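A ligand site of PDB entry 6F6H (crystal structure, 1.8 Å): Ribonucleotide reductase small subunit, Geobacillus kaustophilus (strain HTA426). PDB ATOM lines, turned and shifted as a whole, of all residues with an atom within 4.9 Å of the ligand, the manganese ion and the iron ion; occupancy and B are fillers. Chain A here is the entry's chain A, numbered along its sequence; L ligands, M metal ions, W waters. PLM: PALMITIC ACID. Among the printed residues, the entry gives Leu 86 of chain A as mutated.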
ATOM      1  N   LEU A  75       5.031 -27.554 -14.731  1.00  0.00           N
ATOM      2  CA  LEU A  75       4.362 -26.279 -14.889  1.00  0.00           C
ATOM      3  C   LEU A  75       3.891 -26.090 -16.328  1.00  0.00           C
ATOM      4  O   LEU A  75       2.745 -25.669 -16.548  1.00  0.00           O
ATOM      5  CB  LEU A  75       5.305 -25.145 -14.469  1.00  0.00           C
ATOM      6  CG  LEU A  75       4.658 -23.816 -14.048  1.00  0.00           C
ATOM      7  CD1 LEU A  75       3.770 -24.030 -12.801  1.00  0.00           C
ATOM      8  CD2 LEU A  75       5.707 -22.757 -13.762  1.00  0.00           C
ATOM      9  N   GLY A  78       0.888 -28.170 -17.023  1.00  0.00           N
ATOM     10  CA  GLY A  78      -0.325 -27.625 -16.449  1.00  0.00           C
ATOM     11  C   GLY A  78      -0.893 -26.518 -17.314  1.00  0.00           C
ATOM     12  O   GLY A  78      -2.102 -26.465 -17.554  1.00  0.00           O
ATOM     13  N   PHE A  79      -0.020 -25.625 -17.800  1.00  0.00           N
ATOM     14  CA  PHE A  79      -0.492 -24.553 -18.672  1.00  0.00           C
ATOM     15  C   PHE A  79      -0.979 -25.100 -20.002  1.00  0.00           C
ATOM     16  O   PHE A  79      -2.048 -24.692 -20.482  1.00  0.00           O
ATOM     17  CB  PHE A  79       0.606 -23.523 -18.923  1.00  0.00           C
ATOM     18  CG  PHE A  79       0.551 -22.354 -17.963  1.00  0.00           C
ATOM     19  CD1 PHE A  79      -0.351 -21.319 -18.156  1.00  0.00           C
ATOM     20  CD2 PHE A  79       1.394 -22.308 -16.866  1.00  0.00           C
ATOM     21  CE1 PHE A  79      -0.399 -20.255 -17.243  1.00  0.00           C
ATOM     22  CE2 PHE A  79       1.359 -21.247 -15.971  1.00  0.00           C
ATOM     23  CZ  PHE A  79       0.467 -20.243 -16.157  1.00  0.00           C
ATOM     24  N   GLY A  82      -4.332 -26.480 -19.734  1.00  0.00           N
ATOM     25  CA  GLY A  82      -5.206 -25.359 -19.382  1.00  0.00           C
ATOM     26  C   GLY A  82      -5.589 -24.496 -20.572  1.00  0.00           C
ATOM     27  O   GLY A  82      -6.769 -24.213 -20.796  1.00  0.00           O
ATOM     28  N   GLU A  83      -4.594 -24.035 -21.334  1.00  0.00           N
ATOM     29  CA  GLU A  83      -4.871 -23.238 -22.525  1.00  0.00           C
ATOM     30  C   GLU A  83      -5.797 -23.971 -23.480  1.00  0.00           C
ATOM     31  O   GLU A  83      -6.738 -23.371 -24.051  1.00  0.00           O
ATOM     32  CB  GLU A  83      -3.576 -22.883 -23.274  1.00  0.00           C
ATOM     33  CG  GLU A  83      -2.473 -22.214 -22.438  1.00  0.00           C
ATOM     34  CD  GLU A  83      -2.907 -20.956 -21.687  1.00  0.00           C
ATOM     35  OE1 GLU A  83      -3.959 -20.361 -22.014  1.00  0.00           O
ATOM     36  OE2 GLU A  83      -2.154 -20.531 -20.785  1.00  0.00           O
ATOM     37  N   LEU A  86      -9.311 -24.198 -22.075  1.00  0.00           N
ATOM     38  CA  LEU A  86      -9.972 -22.908 -22.095  1.00  0.00           C
ATOM     39  C   LEU A  86     -10.309 -22.463 -23.508  1.00  0.00           C
ATOM     40  O   LEU A  86     -11.313 -21.777 -23.708  1.00  0.00           O
ATOM     41  CB  LEU A  86      -9.115 -21.875 -21.371  1.00  0.00           C
ATOM     42  CG  LEU A  86      -9.499 -21.740 -19.889  1.00  0.00           C
ATOM     43  CD1 LEU A  86      -9.374 -22.969 -19.093  1.00  0.00           C
ATOM     44  CD2 LEU A  86      -8.616 -20.676 -19.257  1.00  0.00           C
ATOM     45  N   PHE A 112     -11.465 -12.919 -26.611  1.00  0.00           N
ATOM     46  CA  PHE A 112     -11.149 -13.891 -25.560  1.00  0.00           C
ATOM     47  C   PHE A 112     -10.727 -15.234 -26.184  1.00  0.00           C
ATOM     48  O   PHE A 112      -9.668 -15.795 -25.846  1.00  0.00           O
ATOM     49  CB  PHE A 112     -12.400 -14.023 -24.662  1.00  0.00           C
ATOM     50  CG  PHE A 112     -12.169 -14.635 -23.308  1.00  0.00           C
ATOM     51  CD1 PHE A 112     -12.904 -14.222 -22.227  1.00  0.00           C
ATOM     52  CD2 PHE A 112     -11.311 -15.711 -23.130  1.00  0.00           C
ATOM     53  CE1 PHE A 112     -12.708 -14.778 -20.980  1.00  0.00           C
ATOM     54  CE2 PHE A 112     -11.128 -16.279 -21.891  1.00  0.00           C
ATOM     55  CZ  PHE A 112     -11.813 -15.793 -20.806  1.00  0.00           C
ATOM     56  N   GLU A 116      -6.937 -17.249 -26.205  1.00  0.00           N
ATOM     57  CA  GLU A 116      -6.628 -18.569 -25.673  1.00  0.00           C
ATOM     58  C   GLU A 116      -6.031 -19.472 -26.755  1.00  0.00           C
ATOM     59  O   GLU A 116      -5.133 -20.275 -26.470  1.00  0.00           O
ATOM     60  CB  GLU A 116      -7.900 -19.209 -25.066  1.00  0.00           C
ATOM     61  CG  GLU A 116      -8.499 -18.359 -23.923  1.00  0.00           C
ATOM     62  CD  GLU A 116      -7.678 -18.295 -22.643  1.00  0.00           C
ATOM     63  OE1 GLU A 116      -6.532 -18.807 -22.578  1.00  0.00           O
ATOM     64  OE2 GLU A 116      -8.181 -17.680 -21.690  1.00  0.00           O
ATOM     65  N   HIS A 119      -2.504 -18.610 -26.800  1.00  0.00           N
ATOM     66  CA  HIS A 119      -1.855 -19.235 -25.651  1.00  0.00           C
ATOM     67  C   HIS A 119      -1.506 -20.703 -25.908  1.00  0.00           C
ATOM     68  O   HIS A 119      -0.389 -21.144 -25.583  1.00  0.00           O
ATOM     69  CB  HIS A 119      -2.755 -19.097 -24.438  1.00  0.00           C
ATOM     70  CG  HIS A 119      -3.046 -17.679 -24.076  1.00  0.00           C
ATOM     71  ND1 HIS A 119      -3.707 -17.315 -22.916  1.00  0.00           N
ATOM     72  CD2 HIS A 119      -2.719 -16.518 -24.697  1.00  0.00           C
ATOM     73  CE1 HIS A 119      -3.814 -15.992 -22.863  1.00  0.00           C
ATOM     74  NE2 HIS A 119      -3.215 -15.490 -23.929  1.00  0.00           N
ATOM     75  N   TYR A 145      -5.723 -31.970 -10.401  1.00  0.00           N
ATOM     76  CA  TYR A 145      -5.717 -31.260 -11.678  1.00  0.00           C
ATOM     77  C   TYR A 145      -6.834 -31.784 -12.591  1.00  0.00           C
ATOM     78  O   TYR A 145      -7.562 -31.009 -13.216  1.00  0.00           O
ATOM     79  CB  TYR A 145      -4.356 -31.379 -12.341  1.00  0.00           C
ATOM     80  CG  TYR A 145      -4.240 -30.581 -13.589  1.00  0.00           C
ATOM     81  CD1 TYR A 145      -3.704 -29.300 -13.570  1.00  0.00           C
ATOM     82  CD2 TYR A 145      -4.613 -31.100 -14.805  1.00  0.00           C
ATOM     83  CE1 TYR A 145      -3.590 -28.566 -14.715  1.00  0.00           C
ATOM     84  CE2 TYR A 145      -4.512 -30.378 -15.959  1.00  0.00           C
ATOM     85  CZ  TYR A 145      -3.972 -29.105 -15.907  1.00  0.00           C
ATOM     86  OH  TYR A 145      -3.871 -28.368 -17.035  1.00  0.00           O
ATOM     87  N   PHE A 149      -9.659 -29.614 -14.580  1.00  0.00           N
ATOM     88  CA  PHE A 149      -9.549 -29.346 -16.012  1.00  0.00           C
ATOM     89  C   PHE A 149     -10.178 -30.413 -16.915  1.00  0.00           C
ATOM     90  O   PHE A 149     -10.652 -30.085 -18.014  1.00  0.00           O
ATOM     91  CB  PHE A 149      -8.073 -29.180 -16.364  1.00  0.00           C
ATOM     92  CG  PHE A 149      -7.509 -27.873 -15.880  1.00  0.00           C
ATOM     93  CD1 PHE A 149      -7.663 -26.736 -16.634  1.00  0.00           C
ATOM     94  CD2 PHE A 149      -6.862 -27.794 -14.659  1.00  0.00           C
ATOM     95  CE1 PHE A 149      -7.146 -25.528 -16.193  1.00  0.00           C
ATOM     96  CE2 PHE A 149      -6.358 -26.585 -14.222  1.00  0.00           C
ATOM     97  CZ  PHE A 149      -6.502 -25.453 -14.984  1.00  0.00           C
ATOM     98  N   VAL A 180      -9.720 -20.988 -12.434  1.00  0.00           N
ATOM     99  CA  VAL A 180      -8.661 -21.370 -13.381  1.00  0.00           C
ATOM    100  C   VAL A 180      -7.821 -20.163 -13.754  1.00  0.00           C
ATOM    101  O   VAL A 180      -6.587 -20.204 -13.677  1.00  0.00           O
ATOM    102  CB  VAL A 180      -9.256 -22.063 -14.601  1.00  0.00           C
ATOM    103  CG1 VAL A 180      -8.198 -22.304 -15.643  1.00  0.00           C
ATOM    104  CG2 VAL A 180      -9.922 -23.419 -14.161  1.00  0.00           C
ATOM    105  N   GLU A 181      -8.456 -19.077 -14.200  1.00  0.00           N
ATOM    106  CA  GLU A 181      -7.710 -17.889 -14.611  1.00  0.00           C
ATOM    107  C   GLU A 181      -7.232 -17.074 -13.411  1.00  0.00           C
ATOM    108  O   GLU A 181      -6.031 -16.764 -13.277  1.00  0.00           O
ATOM    109  CB  GLU A 181      -8.588 -17.025 -15.528  1.00  0.00           C
ATOM    110  CG  GLU A 181      -8.695 -17.637 -16.914  1.00  0.00           C
ATOM    111  CD  GLU A 181      -9.589 -16.926 -17.888  1.00  0.00           C
ATOM    112  OE1 GLU A 181     -10.611 -16.366 -17.460  1.00  0.00           O
ATOM    113  OE2 GLU A 181      -9.274 -16.959 -19.117  1.00  0.00           O
ATOM    114  N   LEU A 184      -5.279 -20.016 -10.501  1.00  0.00           N
ATOM    115  CA  LEU A 184      -4.187 -20.866 -10.967  1.00  0.00           C
ATOM    116  C   LEU A 184      -3.295 -20.165 -12.010  1.00  0.00           C
ATOM    117  O   LEU A 184      -2.071 -20.157 -11.869  1.00  0.00           O
ATOM    118  CB  LEU A 184      -4.728 -22.170 -11.518  1.00  0.00           C
ATOM    119  CG  LEU A 184      -5.276 -23.113 -10.471  1.00  0.00           C
ATOM    120  CD1 LEU A 184      -5.952 -24.307 -11.195  1.00  0.00           C
ATOM    121  CD2 LEU A 184      -4.156 -23.613  -9.582  1.00  0.00           C
ATOM    122  N   ALA A 185      -3.874 -19.578 -13.067  1.00  0.00           N
ATOM    123  CA  ALA A 185      -3.001 -19.016 -14.109  1.00  0.00           C
ATOM    124  C   ALA A 185      -2.160 -17.898 -13.543  1.00  0.00           C
ATOM    125  O   ALA A 185      -0.966 -17.796 -13.847  1.00  0.00           O
ATOM    126  CB  ALA A 185      -3.784 -18.472 -15.282  1.00  0.00           C
ATOM    127  N   SER A 187      -1.121 -17.465 -10.551  1.00  0.00           N
ATOM    128  CA  SER A 187      -0.091 -17.980  -9.687  1.00  0.00           C
ATOM    129  C   SER A 187       0.970 -18.690 -10.499  1.00  0.00           C
ATOM    130  O   SER A 187       2.144 -18.660 -10.131  1.00  0.00           O
ATOM    131  CB  SER A 187      -0.725 -18.879  -8.615  1.00  0.00           C
ATOM    132  OG  SER A 187      -1.651 -18.130  -7.843  1.00  0.00           O
ATOM    133  N   GLY A 188       0.595 -19.260 -11.653  1.00  0.00           N
ATOM    134  CA  GLY A 188       1.578 -19.792 -12.589  1.00  0.00           C
ATOM    135  C   GLY A 188       2.490 -18.721 -13.169  1.00  0.00           C
ATOM    136  O   GLY A 188       3.706 -18.924 -13.282  1.00  0.00           O
ATOM    137  N   TYR A 189       1.912 -17.597 -13.617  1.00  0.00           N
ATOM    138  CA  TYR A 189       2.750 -16.495 -14.149  1.00  0.00           C
ATOM    139  C   TYR A 189       3.758 -16.061 -13.112  1.00  0.00           C
ATOM    140  O   TYR A 189       4.938 -15.850 -13.415  1.00  0.00           O
ATOM    141  CB  TYR A 189       1.886 -15.290 -14.547  1.00  0.00           C
ATOM    142  CG  TYR A 189       0.828 -15.606 -15.560  1.00  0.00           C
ATOM    143  CD1 TYR A 189       1.072 -16.513 -16.572  1.00  0.00           C
ATOM    144  CD2 TYR A 189      -0.437 -15.005 -15.514  1.00  0.00           C
ATOM    145  CE1 TYR A 189       0.101 -16.838 -17.491  1.00  0.00           C
ATOM    146  CE2 TYR A 189      -1.414 -15.322 -16.412  1.00  0.00           C
ATOM    147  CZ  TYR A 189      -1.140 -16.242 -17.427  1.00  0.00           C
ATOM    148  OH  TYR A 189      -2.104 -16.589 -18.349  1.00  0.00           O
ATOM    149  N   THR A 191       4.884 -17.771 -10.480  1.00  0.00           N
ATOM    150  CA  THR A 191       5.870 -18.824 -10.273  1.00  0.00           C
ATOM    151  C   THR A 191       6.937 -18.831 -11.371  1.00  0.00           C
ATOM    152  O   THR A 191       8.136 -18.971 -11.081  1.00  0.00           O
ATOM    153  CB  THR A 191       5.155 -20.180 -10.200  1.00  0.00           C
ATOM    154  OG1 THR A 191       4.285 -20.208  -9.052  1.00  0.00           O
ATOM    155  CG2 THR A 191       6.130 -21.329 -10.076  1.00  0.00           C
ATOM    156  N   GLU A 216      -4.665 -12.026 -19.734  1.00  0.00           N
ATOM    157  CA  GLU A 216      -5.433 -12.528 -18.586  1.00  0.00           C
ATOM    158  C   GLU A 216      -6.193 -11.430 -17.861  1.00  0.00           C
ATOM    159  O   GLU A 216      -7.278 -11.663 -17.333  1.00  0.00           O
ATOM    160  CB  GLU A 216      -4.515 -13.216 -17.587  1.00  0.00           C
ATOM    161  CG  GLU A 216      -5.144 -14.360 -16.840  1.00  0.00           C
ATOM    162  CD  GLU A 216      -5.506 -15.447 -17.806  1.00  0.00           C
ATOM    163  OE1 GLU A 216      -4.650 -16.295 -18.083  1.00  0.00           O
ATOM    164  OE2 GLU A 216      -6.641 -15.410 -18.319  1.00  0.00           O
ATOM    165  N   HIS A 219      -9.491 -11.278 -19.394  1.00  0.00           N
ATOM    166  CA  HIS A 219     -10.285 -12.479 -19.156  1.00  0.00           C
ATOM    167  C   HIS A 219     -10.903 -12.453 -17.763  1.00  0.00           C
ATOM    168  O   HIS A 219     -12.093 -12.735 -17.580  1.00  0.00           O
ATOM    169  CB  HIS A 219      -9.406 -13.722 -19.374  1.00  0.00           C
ATOM    170  CG  HIS A 219      -8.795 -13.779 -20.734  1.00  0.00           C
ATOM    171  ND1 HIS A 219      -7.979 -14.808 -21.159  1.00  0.00           N
ATOM    172  CD2 HIS A 219      -8.901 -12.926 -21.773  1.00  0.00           C
ATOM    173  CE1 HIS A 219      -7.624 -14.591 -22.419  1.00  0.00           C
ATOM    174  NE2 HIS A 219      -8.155 -13.448 -22.802  1.00  0.00           N
ATOM    175  N   TYR A 255      -3.502 -29.557  -6.139  1.00  0.00           N
ATOM    176  CA  TYR A 255      -2.603 -29.516  -7.284  1.00  0.00           C
ATOM    177  C   TYR A 255      -1.329 -28.749  -6.940  1.00  0.00           C
ATOM    178  O   TYR A 255      -0.220 -29.196  -7.242  1.00  0.00           O
ATOM    179  CB  TYR A 255      -3.299 -28.895  -8.473  1.00  0.00           C
ATOM    180  CG  TYR A 255      -2.411 -28.652  -9.690  1.00  0.00           C
ATOM    181  CD1 TYR A 255      -1.760 -29.680 -10.315  1.00  0.00           C
ATOM    182  CD2 TYR A 255      -2.316 -27.400 -10.239  1.00  0.00           C
ATOM    183  CE1 TYR A 255      -1.007 -29.487 -11.429  1.00  0.00           C
ATOM    184  CE2 TYR A 255      -1.514 -27.177 -11.382  1.00  0.00           C
ATOM    185  CZ  TYR A 255      -0.879 -28.217 -11.961  1.00  0.00           C
ATOM    186  OH  TYR A 255      -0.120 -28.018 -13.093  1.00  0.00           O
ATOM    187  N   VAL A 256      -1.483 -27.607  -6.273  1.00  0.00           N
ATOM    188  CA  VAL A 256      -0.332 -26.776  -5.924  1.00  0.00           C
ATOM    189  C   VAL A 256       0.632 -27.550  -5.018  1.00  0.00           C
ATOM    190  O   VAL A 256       1.843 -27.493  -5.208  1.00  0.00           O
ATOM    191  CB  VAL A 256      -0.814 -25.472  -5.265  1.00  0.00           C
ATOM    192  CG1 VAL A 256       0.311 -24.790  -4.537  1.00  0.00           C
ATOM    193  CG2 VAL A 256      -1.446 -24.541  -6.296  1.00  0.00           C
ATOM    194  N   LEU A 259       2.609 -29.973  -7.250  1.00  0.00           N
ATOM    195  CA  LEU A 259       3.715 -29.271  -7.899  1.00  0.00           C
ATOM    196  C   LEU A 259       4.819 -28.954  -6.891  1.00  0.00           C
ATOM    197  O   LEU A 259       6.000 -29.027  -7.224  1.00  0.00           O
ATOM    198  CB  LEU A 259       3.235 -27.976  -8.531  1.00  0.00           C
ATOM    199  CG  LEU A 259       2.354 -28.118  -9.764  1.00  0.00           C
ATOM    200  CD1 LEU A 259       1.839 -26.730 -10.133  1.00  0.00           C
ATOM    201  CD2 LEU A 259       3.112 -28.757 -10.906  1.00  0.00           C
ATOM    202  N   THR A 260       4.442 -28.559  -5.677  1.00  0.00           N
ATOM    203  CA  THR A 260       5.427 -28.189  -4.676  1.00  0.00           C
ATOM    204  C   THR A 260       6.298 -29.376  -4.293  1.00  0.00           C
ATOM    205  O   THR A 260       7.531 -29.283  -4.225  1.00  0.00           O
ATOM    206  CB  THR A 260       4.703 -27.636  -3.457  1.00  0.00           C
ATOM    207  OG1 THR A 260       4.179 -26.348  -3.778  1.00  0.00           O
ATOM    208  CG2 THR A 260       5.643 -27.499  -2.291  1.00  0.00           C
ATOM    209  N   TYR A 279       9.044 -22.077  -1.780  1.00  0.00           N
ATOM    210  CA  TYR A 279       7.763 -22.701  -2.111  1.00  0.00           C
ATOM    211  C   TYR A 279       6.677 -22.314  -1.128  1.00  0.00           C
ATOM    212  O   TYR A 279       5.504 -22.263  -1.498  1.00  0.00           O
ATOM    213  CB  TYR A 279       7.891 -24.207  -2.161  1.00  0.00           C
ATOM    214  CG  TYR A 279       8.671 -24.679  -3.328  1.00  0.00           C
ATOM    215  CD1 TYR A 279       8.140 -24.617  -4.614  1.00  0.00           C
ATOM    216  CD2 TYR A 279       9.965 -25.187  -3.165  1.00  0.00           C
ATOM    217  CE1 TYR A 279       8.868 -25.037  -5.699  1.00  0.00           C
ATOM    218  CE2 TYR A 279      10.690 -25.610  -4.241  1.00  0.00           C
ATOM    219  CZ  TYR A 279      10.158 -25.533  -5.501  1.00  0.00           C
ATOM    220  OH  TYR A 279      10.910 -25.957  -6.568  1.00  0.00           O
ATOM    221  N   LEU A 282       5.277 -19.256  -2.590  1.00  0.00           N
ATOM    222  CA  LEU A 282       4.408 -19.490  -3.723  1.00  0.00           C
ATOM    223  C   LEU A 282       3.050 -19.987  -3.274  1.00  0.00           C
ATOM    224  O   LEU A 282       2.021 -19.517  -3.768  1.00  0.00           O
ATOM    225  CB  LEU A 282       5.056 -20.488  -4.691  1.00  0.00           C
ATOM    226  CG  LEU A 282       6.348 -19.966  -5.322  1.00  0.00           C
ATOM    227  CD1 LEU A 282       7.034 -21.001  -6.144  1.00  0.00           C
ATOM    228  CD2 LEU A 282       6.123 -18.710  -6.168  1.00  0.00           C
ATOM    229  N   VAL A 286      -0.841 -18.197  -3.882  1.00  0.00           N
ATOM    230  CA  VAL A 286      -2.051 -18.861  -4.395  1.00  0.00           C
ATOM    231  C   VAL A 286      -3.233 -18.619  -3.474  1.00  0.00           C
ATOM    232  O   VAL A 286      -4.312 -18.204  -3.923  1.00  0.00           O
ATOM    233  CB  VAL A 286      -1.787 -20.361  -4.581  1.00  0.00           C
ATOM    234  CG1 VAL A 286      -3.095 -21.106  -4.953  1.00  0.00           C
ATOM    235  CG2 VAL A 286      -0.740 -20.573  -5.652  1.00  0.00           C
HETATM  236  C1  PLM L   1      -5.729 -19.450 -19.129  1.00  0.00           C
HETATM  237  O1  PLM L   1      -5.271 -19.859 -20.230  1.00  0.00           O
HETATM  238  O2  PLM L   1      -6.407 -18.387 -18.865  1.00  0.00           O
HETATM  239  C2  PLM L   1      -5.528 -20.396 -17.927  1.00  0.00           C
HETATM  240  C3  PLM L   1      -4.520 -21.518 -18.079  1.00  0.00           C
HETATM  241  C4  PLM L   1      -4.546 -22.493 -16.877  1.00  0.00           C
HETATM  242  C5  PLM L   1      -3.202 -22.696 -16.203  1.00  0.00           C
HETATM  243  C6  PLM L   1      -3.162 -23.797 -15.163  1.00  0.00           C
HETATM  244  C7  PLM L   1      -1.741 -24.188 -14.750  1.00  0.00           C
HETATM  245  C8  PLM L   1      -1.089 -23.206 -13.828  1.00  0.00           C
HETATM  246  C9  PLM L   1      -0.147 -23.803 -12.787  1.00  0.00           C
HETATM  247  CA  PLM L   1      -0.423 -23.278 -11.373  1.00  0.00           C
HETATM  248  CB  PLM L   1       0.821 -23.144 -10.559  1.00  0.00           C
HETATM  249  CC  PLM L   1       0.558 -22.622  -9.163  1.00  0.00           C
HETATM  250  CD  PLM L   1       1.835 -22.443  -8.325  1.00  0.00           C
HETATM  251  CE  PLM L   1       2.471 -23.727  -7.821  1.00  0.00           C
HETATM  252  CF  PLM L   1       3.774 -23.542  -7.061  1.00  0.00           C
HETATM  253  CG  PLM L   1       4.841 -24.594  -7.370  1.00  0.00           C
HETATM  254 MN    MN M   1      -4.805 -18.591 -21.375  1.00  0.00          MN
HETATM  255 FE    FE M   2      -7.409 -16.706 -20.029  1.00  0.00          FE
HETATM  256  O   HOH W   1      -5.317 -16.721 -20.504  1.00  0.00           O
HETATM  257  O   HOH W   2      -2.890 -18.564 -20.089  1.00  0.00           O
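The side-chain carboxylate (OE1) of Glu 216 is in hydrogen-bond range of the side-chain hydroxyl (OH) of Tyr 189, at 2.6 Å. OG1 of Thr 191 is in hydrogen-bond range of O of Ser 187 (2.9 Å). The backbone carbonyl oxygen (O) of Gly 78 sits at hydrogen-bond distance from the side-chain hydroxyl (OH) of Tyr 145, 2.6 Å away. The backbone NH (N) of Ala 185 sits at hydrogen-bond distance from the backbone carbonyl oxygen (O) of Val 180 (2.9 Å). The backbone NH of Gly 82 sits at hydrogen-bond distance from the side-chain hydroxyl of Tyr 145 (3.3 Å). The backbone carbonyl oxygen of Val 256 sits at hydrogen-bond distance from the side-chain hydroxyl of Thr 260 (3.0 Å).
Leu 75 touches the ligand. Gly 78 touches the ligand (C to C7, 3.6 Å). CD1 of Phe 79 touches C5 of the ligand (3.7 Å). Gly 82 touches the ligand. Leu 86 touches the ligand. Phe 149 touches the ligand (CZ to C6, 3.7 Å). CG1 of Val 180 touches C4 of the ligand (3.9 Å). Leu 184 touches the ligand. CB of Ala 185 touches C2 of the ligand, at 3.7 Å. Ser 187 touches the ligand. Gly 188 touches the ligand. OG1 of Thr 191 touches CD of the ligand, at 3.4 Å. CE2 of Tyr 255 touches C9 of the ligand (3.9 Å). CG2 of Val 256 touches CC of the ligand, at 3.99 Å. Leu 259 touches the ligand. Hydrophobic or aromatic side chains within 4 Å of the ligand: Leu 75, Phe 79, Leu 86, Phe 149, Val 180, Ala 185, Tyr 255, Val 256 and Leu 259.
Three residues have an atom within 4 Å of the manganese ion: Glu 83, Glu 116 and His 119. The nearest printed residue that does not touch the manganese ion is Glu 216 (4.02 Å).
The manganese ion is bound by O1 of the ligand (1.8 Å), OE1 of Glu 83 (2.1 Å), OE1 of Glu 116 (2.1 Å), water W1 (2.1 Å), ND1 of His 119 (2.3 Å) and water W2 (2.3 Å).
The iron ion is bound by the side-chain carboxylate (OE2) of Glu 116. The iron ion is bound by OE2 of Glu 181 (2.1 Å). Water W1 binds the iron ion. O2 of the ligand binds the iron ion. OE2 of Glu 216 is bound to the iron ion (2.3 Å). The iron ion is bound by ND1 of His 219 (2.3 Å).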
